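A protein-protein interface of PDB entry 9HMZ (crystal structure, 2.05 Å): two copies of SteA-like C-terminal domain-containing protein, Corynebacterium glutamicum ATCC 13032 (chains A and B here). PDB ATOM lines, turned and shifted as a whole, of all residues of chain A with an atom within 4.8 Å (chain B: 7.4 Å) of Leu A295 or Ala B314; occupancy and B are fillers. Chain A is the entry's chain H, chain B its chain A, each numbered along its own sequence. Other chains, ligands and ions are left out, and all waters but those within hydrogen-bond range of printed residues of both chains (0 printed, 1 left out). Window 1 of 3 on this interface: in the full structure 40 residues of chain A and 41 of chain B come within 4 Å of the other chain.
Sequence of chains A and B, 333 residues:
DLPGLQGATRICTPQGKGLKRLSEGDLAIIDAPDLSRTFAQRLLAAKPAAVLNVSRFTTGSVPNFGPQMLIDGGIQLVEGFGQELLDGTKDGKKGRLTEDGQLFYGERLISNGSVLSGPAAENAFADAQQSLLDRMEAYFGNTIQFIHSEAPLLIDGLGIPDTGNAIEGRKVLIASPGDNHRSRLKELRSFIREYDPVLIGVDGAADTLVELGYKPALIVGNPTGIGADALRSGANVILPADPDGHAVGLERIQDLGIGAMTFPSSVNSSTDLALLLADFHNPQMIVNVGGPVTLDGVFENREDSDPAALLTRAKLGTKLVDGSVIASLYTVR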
ATOM      1  N   VAL A 293     -19.364 -28.588 -23.210  1.00  0.00           N
ATOM      2  CA  VAL A 293     -20.424 -27.959 -23.978  1.00  0.00           C
ATOM      3  C   VAL A 293     -20.373 -26.472 -23.619  1.00  0.00           C
ATOM      4  O   VAL A 293     -20.396 -26.126 -22.425  1.00  0.00           O
ATOM      5  CB  VAL A 293     -21.812 -28.616 -23.695  1.00  0.00           C
ATOM      6  CG1 VAL A 293     -22.951 -27.676 -24.063  1.00  0.00           C
ATOM      7  CG2 VAL A 293     -21.951 -29.954 -24.430  1.00  0.00           C
ATOM      8  N   THR A 294     -20.170 -25.611 -24.648  1.00  0.00           N
ATOM      9  CA  THR A 294     -20.065 -24.167 -24.463  1.00  0.00           C
ATOM     10  C   THR A 294     -21.047 -23.365 -25.349  1.00  0.00           C
ATOM     11  O   THR A 294     -21.546 -23.887 -26.341  1.00  0.00           O
ATOM     12  CB  THR A 294     -18.608 -23.699 -24.668  1.00  0.00           C
ATOM     13  OG1 THR A 294     -18.266 -23.703 -26.072  1.00  0.00           O
ATOM     14  CG2 THR A 294     -17.605 -24.506 -23.835  1.00  0.00           C
ATOM     15  N   LEU A 295     -21.307 -22.085 -24.988  1.00  0.00           N
ATOM     16  CA  LEU A 295     -22.169 -21.220 -25.795  1.00  0.00           C
ATOM     17  C   LEU A 295     -21.531 -20.967 -27.169  1.00  0.00           C
ATOM     18  O   LEU A 295     -22.230 -20.945 -28.179  1.00  0.00           O
ATOM     19  CB  LEU A 295     -22.432 -19.875 -25.109  1.00  0.00           C
ATOM     20  CG  LEU A 295     -23.460 -18.982 -25.810  1.00  0.00           C
ATOM     21  CD1 LEU A 295     -24.825 -19.608 -25.762  1.00  0.00           C
ATOM     22  CD2 LEU A 295     -23.503 -17.595 -25.183  1.00  0.00           C
ATOM     23  N   ASP A 296     -20.210 -20.781 -27.202  1.00  0.00           N
ATOM     24  CA  ASP A 296     -19.489 -20.569 -28.450  1.00  0.00           C
ATOM     25  C   ASP A 296     -19.623 -21.773 -29.385  1.00  0.00           C
ATOM     26  O   ASP A 296     -19.787 -21.580 -30.569  1.00  0.00           O
ATOM     27  CB  ASP A 296     -18.018 -20.178 -28.205  1.00  0.00           C
ATOM     28  CG  ASP A 296     -17.835 -18.763 -27.659  1.00  0.00           C
ATOM     29  OD1 ASP A 296     -18.496 -17.825 -28.184  1.00  0.00           O
ATOM     30  OD2 ASP A 296     -17.021 -18.588 -26.715  1.00  0.00           O
ATOM     31  N   GLY A 297     -19.686 -22.977 -28.833  1.00  0.00           N
ATOM     32  CA  GLY A 297     -19.946 -24.185 -29.597  1.00  0.00           C
ATOM     33  C   GLY A 297     -21.326 -24.174 -30.231  1.00  0.00           C
ATOM     34  O   GLY A 297     -21.484 -24.622 -31.363  1.00  0.00           O
ATOM     35  N   VAL A 298     -22.331 -23.642 -29.532  1.00  0.00           N
ATOM     36  CA  VAL A 298     -23.703 -23.500 -30.041  1.00  0.00           C
ATOM     37  C   VAL A 298     -23.736 -22.457 -31.176  1.00  0.00           C
ATOM     38  O   VAL A 298     -24.327 -22.700 -32.231  1.00  0.00           O
ATOM     39  CB  VAL A 298     -24.687 -23.125 -28.895  1.00  0.00           C
ATOM     40  CG1 VAL A 298     -26.050 -22.739 -29.433  1.00  0.00           C
ATOM     41  CG2 VAL A 298     -24.805 -24.247 -27.867  1.00  0.00           C
ATOM     42  N   PHE A 299     -23.077 -21.316 -30.973  1.00  0.00           N
ATOM     43  CA  PHE A 299     -23.007 -20.254 -31.972  1.00  0.00           C
ATOM     44  C   PHE A 299     -22.272 -20.704 -33.242  1.00  0.00           C
ATOM     45  O   PHE A 299     -22.604 -20.261 -34.338  1.00  0.00           O
ATOM     46  CB  PHE A 299     -22.255 -19.039 -31.404  1.00  0.00           C
ATOM     47  CG  PHE A 299     -22.979 -18.181 -30.403  1.00  0.00           C
ATOM     48  CD1 PHE A 299     -24.336 -18.320 -30.201  1.00  0.00           C
ATOM     49  CD2 PHE A 299     -22.305 -17.213 -29.683  1.00  0.00           C
ATOM     50  CE1 PHE A 299     -25.005 -17.513 -29.287  1.00  0.00           C
ATOM     51  CE2 PHE A 299     -22.975 -16.409 -28.769  1.00  0.00           C
ATOM     52  CZ  PHE A 299     -24.322 -16.558 -28.586  1.00  0.00           C
ATOM     53  N   LEU A 310     -26.761 -27.839 -22.895  1.00  0.00           N
ATOM     54  CA  LEU A 310     -26.500 -26.572 -22.215  1.00  0.00           C
ATOM     55  C   LEU A 310     -27.413 -26.429 -20.998  1.00  0.00           C
ATOM     56  O   LEU A 310     -26.973 -25.891 -19.982  1.00  0.00           O
ATOM     57  CB  LEU A 310     -26.670 -25.386 -23.193  1.00  0.00           C
ATOM     58  CG  LEU A 310     -25.713 -24.180 -23.057  1.00  0.00           C
ATOM     59  CD1 LEU A 310     -24.239 -24.634 -22.977  1.00  0.00           C
ATOM     60  CD2 LEU A 310     -25.904 -23.213 -24.216  1.00  0.00           C
ATOM     61  N   THR B 143     -33.640 -13.732 -24.365  1.00  0.00           N
ATOM     62  CA  THR B 143     -32.317 -14.301 -24.625  1.00  0.00           C
ATOM     63  C   THR B 143     -32.012 -14.191 -26.116  1.00  0.00           C
ATOM     64  O   THR B 143     -30.916 -13.773 -26.473  1.00  0.00           O
ATOM     65  CB  THR B 143     -32.246 -15.753 -24.144  1.00  0.00           C
ATOM     66  OG1 THR B 143     -32.543 -15.803 -22.749  1.00  0.00           O
ATOM     67  CG2 THR B 143     -30.893 -16.381 -24.390  1.00  0.00           C
ATOM     68  N   ILE B 147     -29.009 -11.854 -27.723  1.00  0.00           N
ATOM     69  CA  ILE B 147     -27.972 -12.364 -28.624  1.00  0.00           C
ATOM     70  C   ILE B 147     -27.944 -11.570 -29.921  1.00  0.00           C
ATOM     71  O   ILE B 147     -26.871 -11.221 -30.406  1.00  0.00           O
ATOM     72  CB  ILE B 147     -28.151 -13.880 -28.892  1.00  0.00           C
ATOM     73  CG1 ILE B 147     -27.954 -14.679 -27.597  1.00  0.00           C
ATOM     74  CG2 ILE B 147     -27.177 -14.357 -29.971  1.00  0.00           C
ATOM     75  CD1 ILE B 147     -28.342 -16.085 -27.713  1.00  0.00           C
ATOM     76  N   LEU B 154     -20.845 -10.351 -27.583  1.00  0.00           N
ATOM     77  CA  LEU B 154     -20.706 -11.785 -27.385  1.00  0.00           C
ATOM     78  C   LEU B 154     -19.763 -12.466 -28.363  1.00  0.00           C
ATOM     79  O   LEU B 154     -19.113 -13.433 -27.983  1.00  0.00           O
ATOM     80  CB  LEU B 154     -22.077 -12.447 -27.478  1.00  0.00           C
ATOM     81  CG  LEU B 154     -23.033 -12.152 -26.334  1.00  0.00           C
ATOM     82  CD1 LEU B 154     -24.412 -12.680 -26.662  1.00  0.00           C
ATOM     83  CD2 LEU B 154     -22.495 -12.745 -25.007  1.00  0.00           C
ATOM     84  N   ILE B 155     -19.710 -12.008 -29.618  1.00  0.00           N
ATOM     85  CA  ILE B 155     -18.887 -12.604 -30.658  1.00  0.00           C
ATOM     86  C   ILE B 155     -17.551 -11.901 -30.770  1.00  0.00           C
ATOM     87  O   ILE B 155     -16.522 -12.563 -30.739  1.00  0.00           O
ATOM     88  CB  ILE B 155     -19.632 -12.608 -32.040  1.00  0.00           C
ATOM     89  CG1 ILE B 155     -20.958 -13.400 -31.994  1.00  0.00           C
ATOM     90  CG2 ILE B 155     -18.732 -13.078 -33.203  1.00  0.00           C
ATOM     91  CD1 ILE B 155     -20.806 -14.771 -31.715  1.00  0.00           C
ATOM     92  N   ALA B 308     -28.704 -12.061 -19.591  1.00  0.00           N
ATOM     93  CA  ALA B 308     -27.296 -11.731 -19.730  1.00  0.00           C
ATOM     94  C   ALA B 308     -26.440 -12.471 -18.710  1.00  0.00           C
ATOM     95  O   ALA B 308     -25.321 -12.852 -19.031  1.00  0.00           O
ATOM     96  CB  ALA B 308     -27.086 -10.235 -19.613  1.00  0.00           C
ATOM     97  N   ALA B 309     -26.964 -12.714 -17.507  1.00  0.00           N
ATOM     98  CA  ALA B 309     -26.261 -13.437 -16.453  1.00  0.00           C
ATOM     99  C   ALA B 309     -25.998 -14.917 -16.820  1.00  0.00           C
ATOM    100  O   ALA B 309     -24.851 -15.354 -16.775  1.00  0.00           O
ATOM    101  CB  ALA B 309     -27.030 -13.325 -15.135  1.00  0.00           C
ATOM    102  N   LEU B 310     -27.027 -15.668 -17.230  1.00  0.00           N
ATOM    103  CA  LEU B 310     -26.859 -17.063 -17.613  1.00  0.00           C
ATOM    104  C   LEU B 310     -26.109 -17.179 -18.932  1.00  0.00           C
ATOM    105  O   LEU B 310     -25.319 -18.108 -19.079  1.00  0.00           O
ATOM    106  CB  LEU B 310     -28.237 -17.762 -17.678  1.00  0.00           C
ATOM    107  CG  LEU B 310     -28.328 -19.225 -17.192  1.00  0.00           C
ATOM    108  CD1 LEU B 310     -27.722 -19.396 -15.791  1.00  0.00           C
ATOM    109  CD2 LEU B 310     -29.743 -19.691 -17.179  1.00  0.00           C
ATOM    110  N   LEU B 311     -26.301 -16.235 -19.875  1.00  0.00           N
ATOM    111  CA  LEU B 311     -25.540 -16.256 -21.137  1.00  0.00           C
ATOM    112  C   LEU B 311     -24.058 -16.014 -20.865  1.00  0.00           C
ATOM    113  O   LEU B 311     -23.229 -16.599 -21.554  1.00  0.00           O
ATOM    114  CB  LEU B 311     -26.020 -15.204 -22.154  1.00  0.00           C
ATOM    115  CG  LEU B 311     -27.217 -15.564 -23.027  1.00  0.00           C
ATOM    116  CD1 LEU B 311     -27.658 -14.386 -23.843  1.00  0.00           C
ATOM    117  CD2 LEU B 311     -26.928 -16.733 -23.919  1.00  0.00           C
ATOM    118  N   THR B 312     -23.724 -15.153 -19.877  1.00  0.00           N
ATOM    119  CA  THR B 312     -22.329 -14.886 -19.499  1.00  0.00           C
ATOM    120  C   THR B 312     -21.661 -16.148 -18.963  1.00  0.00           C
ATOM    121  O   THR B 312     -20.541 -16.459 -19.358  1.00  0.00           O
ATOM    122  CB  THR B 312     -22.226 -13.737 -18.489  1.00  0.00           C
ATOM    123  OG1 THR B 312     -22.767 -12.571 -19.085  1.00  0.00           O
ATOM    124  CG2 THR B 312     -20.802 -13.466 -18.062  1.00  0.00           C
ATOM    125  N   ARG B 313     -22.355 -16.904 -18.103  1.00  0.00           N
ATOM    126  CA  ARG B 313     -21.817 -18.137 -17.555  1.00  0.00           C
ATOM    127  C   ARG B 313     -21.563 -19.150 -18.663  1.00  0.00           C
ATOM    128  O   ARG B 313     -20.539 -19.844 -18.638  1.00  0.00           O
ATOM    129  CB  ARG B 313     -22.765 -18.733 -16.487  1.00  0.00           C
ATOM    130  CG  ARG B 313     -23.212 -17.770 -15.366  1.00  0.00           C
ATOM    131  CD  ARG B 313     -22.046 -17.067 -14.707  1.00  0.00           C
ATOM    132  NE  ARG B 313     -22.382 -16.315 -13.497  1.00  0.00           N
ATOM    133  CZ  ARG B 313     -22.780 -15.046 -13.479  1.00  0.00           C
ATOM    134  NH1 ARG B 313     -22.994 -14.397 -14.612  1.00  0.00           N
ATOM    135  NH2 ARG B 313     -22.984 -14.425 -12.326  1.00  0.00           N
ATOM    136  N   ALA B 314     -22.492 -19.238 -19.643  1.00  0.00           N
ATOM    137  CA  ALA B 314     -22.372 -20.172 -20.765  1.00  0.00           C
ATOM    138  C   ALA B 314     -21.242 -19.740 -21.739  1.00  0.00           C
ATOM    139  O   ALA B 314     -20.531 -20.587 -22.278  1.00  0.00           O
ATOM    140  CB  ALA B 314     -23.698 -20.270 -21.494  1.00  0.00           C
ATOM    141  N   LYS B 315     -21.062 -18.425 -21.918  1.00  0.00           N
ATOM    142  CA  LYS B 315     -20.033 -17.820 -22.759  1.00  0.00           C
ATOM    143  C   LYS B 315     -18.644 -18.201 -22.236  1.00  0.00           C
ATOM    144  O   LYS B 315     -17.775 -18.568 -23.030  1.00  0.00           O
ATOM    145  CB  LYS B 315     -20.220 -16.278 -22.765  1.00  0.00           C
ATOM    146  CG  LYS B 315     -19.063 -15.473 -23.355  1.00  0.00           C
ATOM    147  CD  LYS B 315     -18.892 -15.726 -24.818  1.00  0.00           C
ATOM    148  CE  LYS B 315     -17.648 -15.048 -25.309  1.00  0.00           C
ATOM    149  NZ  LYS B 315     -17.420 -15.288 -26.752  1.00  0.00           N
ATOM    150  N   LEU B 316     -18.427 -18.110 -20.903  1.00  0.00           N
ATOM    151  CA  LEU B 316     -17.150 -18.475 -20.278  1.00  0.00           C
ATOM    152  C   LEU B 316     -16.849 -19.968 -20.406  1.00  0.00           C
ATOM    153  O   LEU B 316     -15.685 -20.363 -20.388  1.00  0.00           O
ATOM    154  CB  LEU B 316     -17.121 -18.055 -18.819  1.00  0.00           C
ATOM    155  CG  LEU B 316     -16.585 -16.658 -18.506  1.00  0.00           C
ATOM    156  CD1 LEU B 316     -17.346 -15.565 -19.263  1.00  0.00           C
ATOM    157  CD2 LEU B 316     -16.677 -16.388 -17.028  1.00  0.00           C
ATOM    158  N   GLY B 317     -17.898 -20.780 -20.542  1.00  0.00           N
ATOM    159  CA  GLY B 317     -17.821 -22.216 -20.780  1.00  0.00           C
ATOM    160  C   GLY B 317     -17.015 -22.978 -19.760  1.00  0.00           C
ATOM    161  O   GLY B 317     -17.225 -22.821 -18.553  1.00  0.00           O
ATOM    162  N   THR B 318     -16.049 -23.761 -20.261  1.00  0.00           N
ATOM    163  CA  THR B 318     -15.218 -24.634 -19.462  1.00  0.00           C
ATOM    164  C   THR B 318     -14.216 -23.924 -18.576  1.00  0.00           C
ATOM    165  O   THR B 318     -13.688 -24.560 -17.676  1.00  0.00           O
ATOM    166  CB  THR B 318     -14.522 -25.665 -20.361  1.00  0.00           C
ATOM    167  OG1 THR B 318     -13.633 -24.991 -21.258  1.00  0.00           O
ATOM    168  CG2 THR B 318     -15.507 -26.532 -21.114  1.00  0.00           C
ATOM    169  N   LEU B 320     -14.866 -21.396 -16.475  1.00  0.00           N
ATOM    170  CA  LEU B 320     -15.533 -20.974 -15.259  1.00  0.00           C
ATOM    171  C   LEU B 320     -15.575 -22.029 -14.137  1.00  0.00           C
ATOM    172  O   LEU B 320     -15.962 -23.168 -14.362  1.00  0.00           O
ATOM    173  CB  LEU B 320     -16.953 -20.508 -15.602  1.00  0.00           C
ATOM    174  CG  LEU B 320     -17.814 -19.958 -14.433  1.00  0.00           C
ATOM    175  CD1 LEU B 320     -17.277 -18.667 -13.917  1.00  0.00           C
ATOM    176  CD2 LEU B 320     -19.249 -19.795 -14.858  1.00  0.00           C
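O of Ala B314 is in hydrogen-bond range of N of Leu A295, at 3.2 Å. NZ of Lys B315 lies within salt-bridge range of OD1 of Asp A296 (3.1 Å).
N of Gly A297 is in hydrogen-bond range of OG1 of Thr A294, at 3.2 Å. The backbone carbonyl oxygen (O) of Leu B154 sits at hydrogen-bond distance from the side-chain amino group (NZ) of Lys B315 (2.8 Å).
Among the printed residues, pairs that only touch across the chains: Thr A294 with Gly B317, Thr A294 with Thr B318, Leu A295 with Leu B311, Leu A295 with Lys B315, Phe A299 with Ile B147 and Phe A299 with Ile B155.
Of chain B, only Leu B311 (3.8 Å), Ala B314 (3.2 Å) and Lys B315 (3.8 Å) come within 4 Å of Leu A295. Of chain A, only Leu A295 comes within 4 Å of Ala B314. Of the printed residues of chain A, Ile B155 touches Phe A299. Of the printed residues of chain B, Phe A299 touches Ile B147 (3.9 Å) and Ile B155 (3.5 Å). Printed residues of chain A within 4 Å of Ile B147: Phe A299. Of the printed residues of chain B, Thr A294 touches Gly B317 (3.8 Å) and Thr B318 (3.97 Å). Leu B154 touches none of the printed residues of chain A.
Of the 8 printed residues of chain A, 4 touch a printed residue of chain B. Hydrophobic or aromatic side chains of chain A within 4 Å of the printed part of chain B: Leu A295 and Phe A299.
1 position is printed for both chains.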
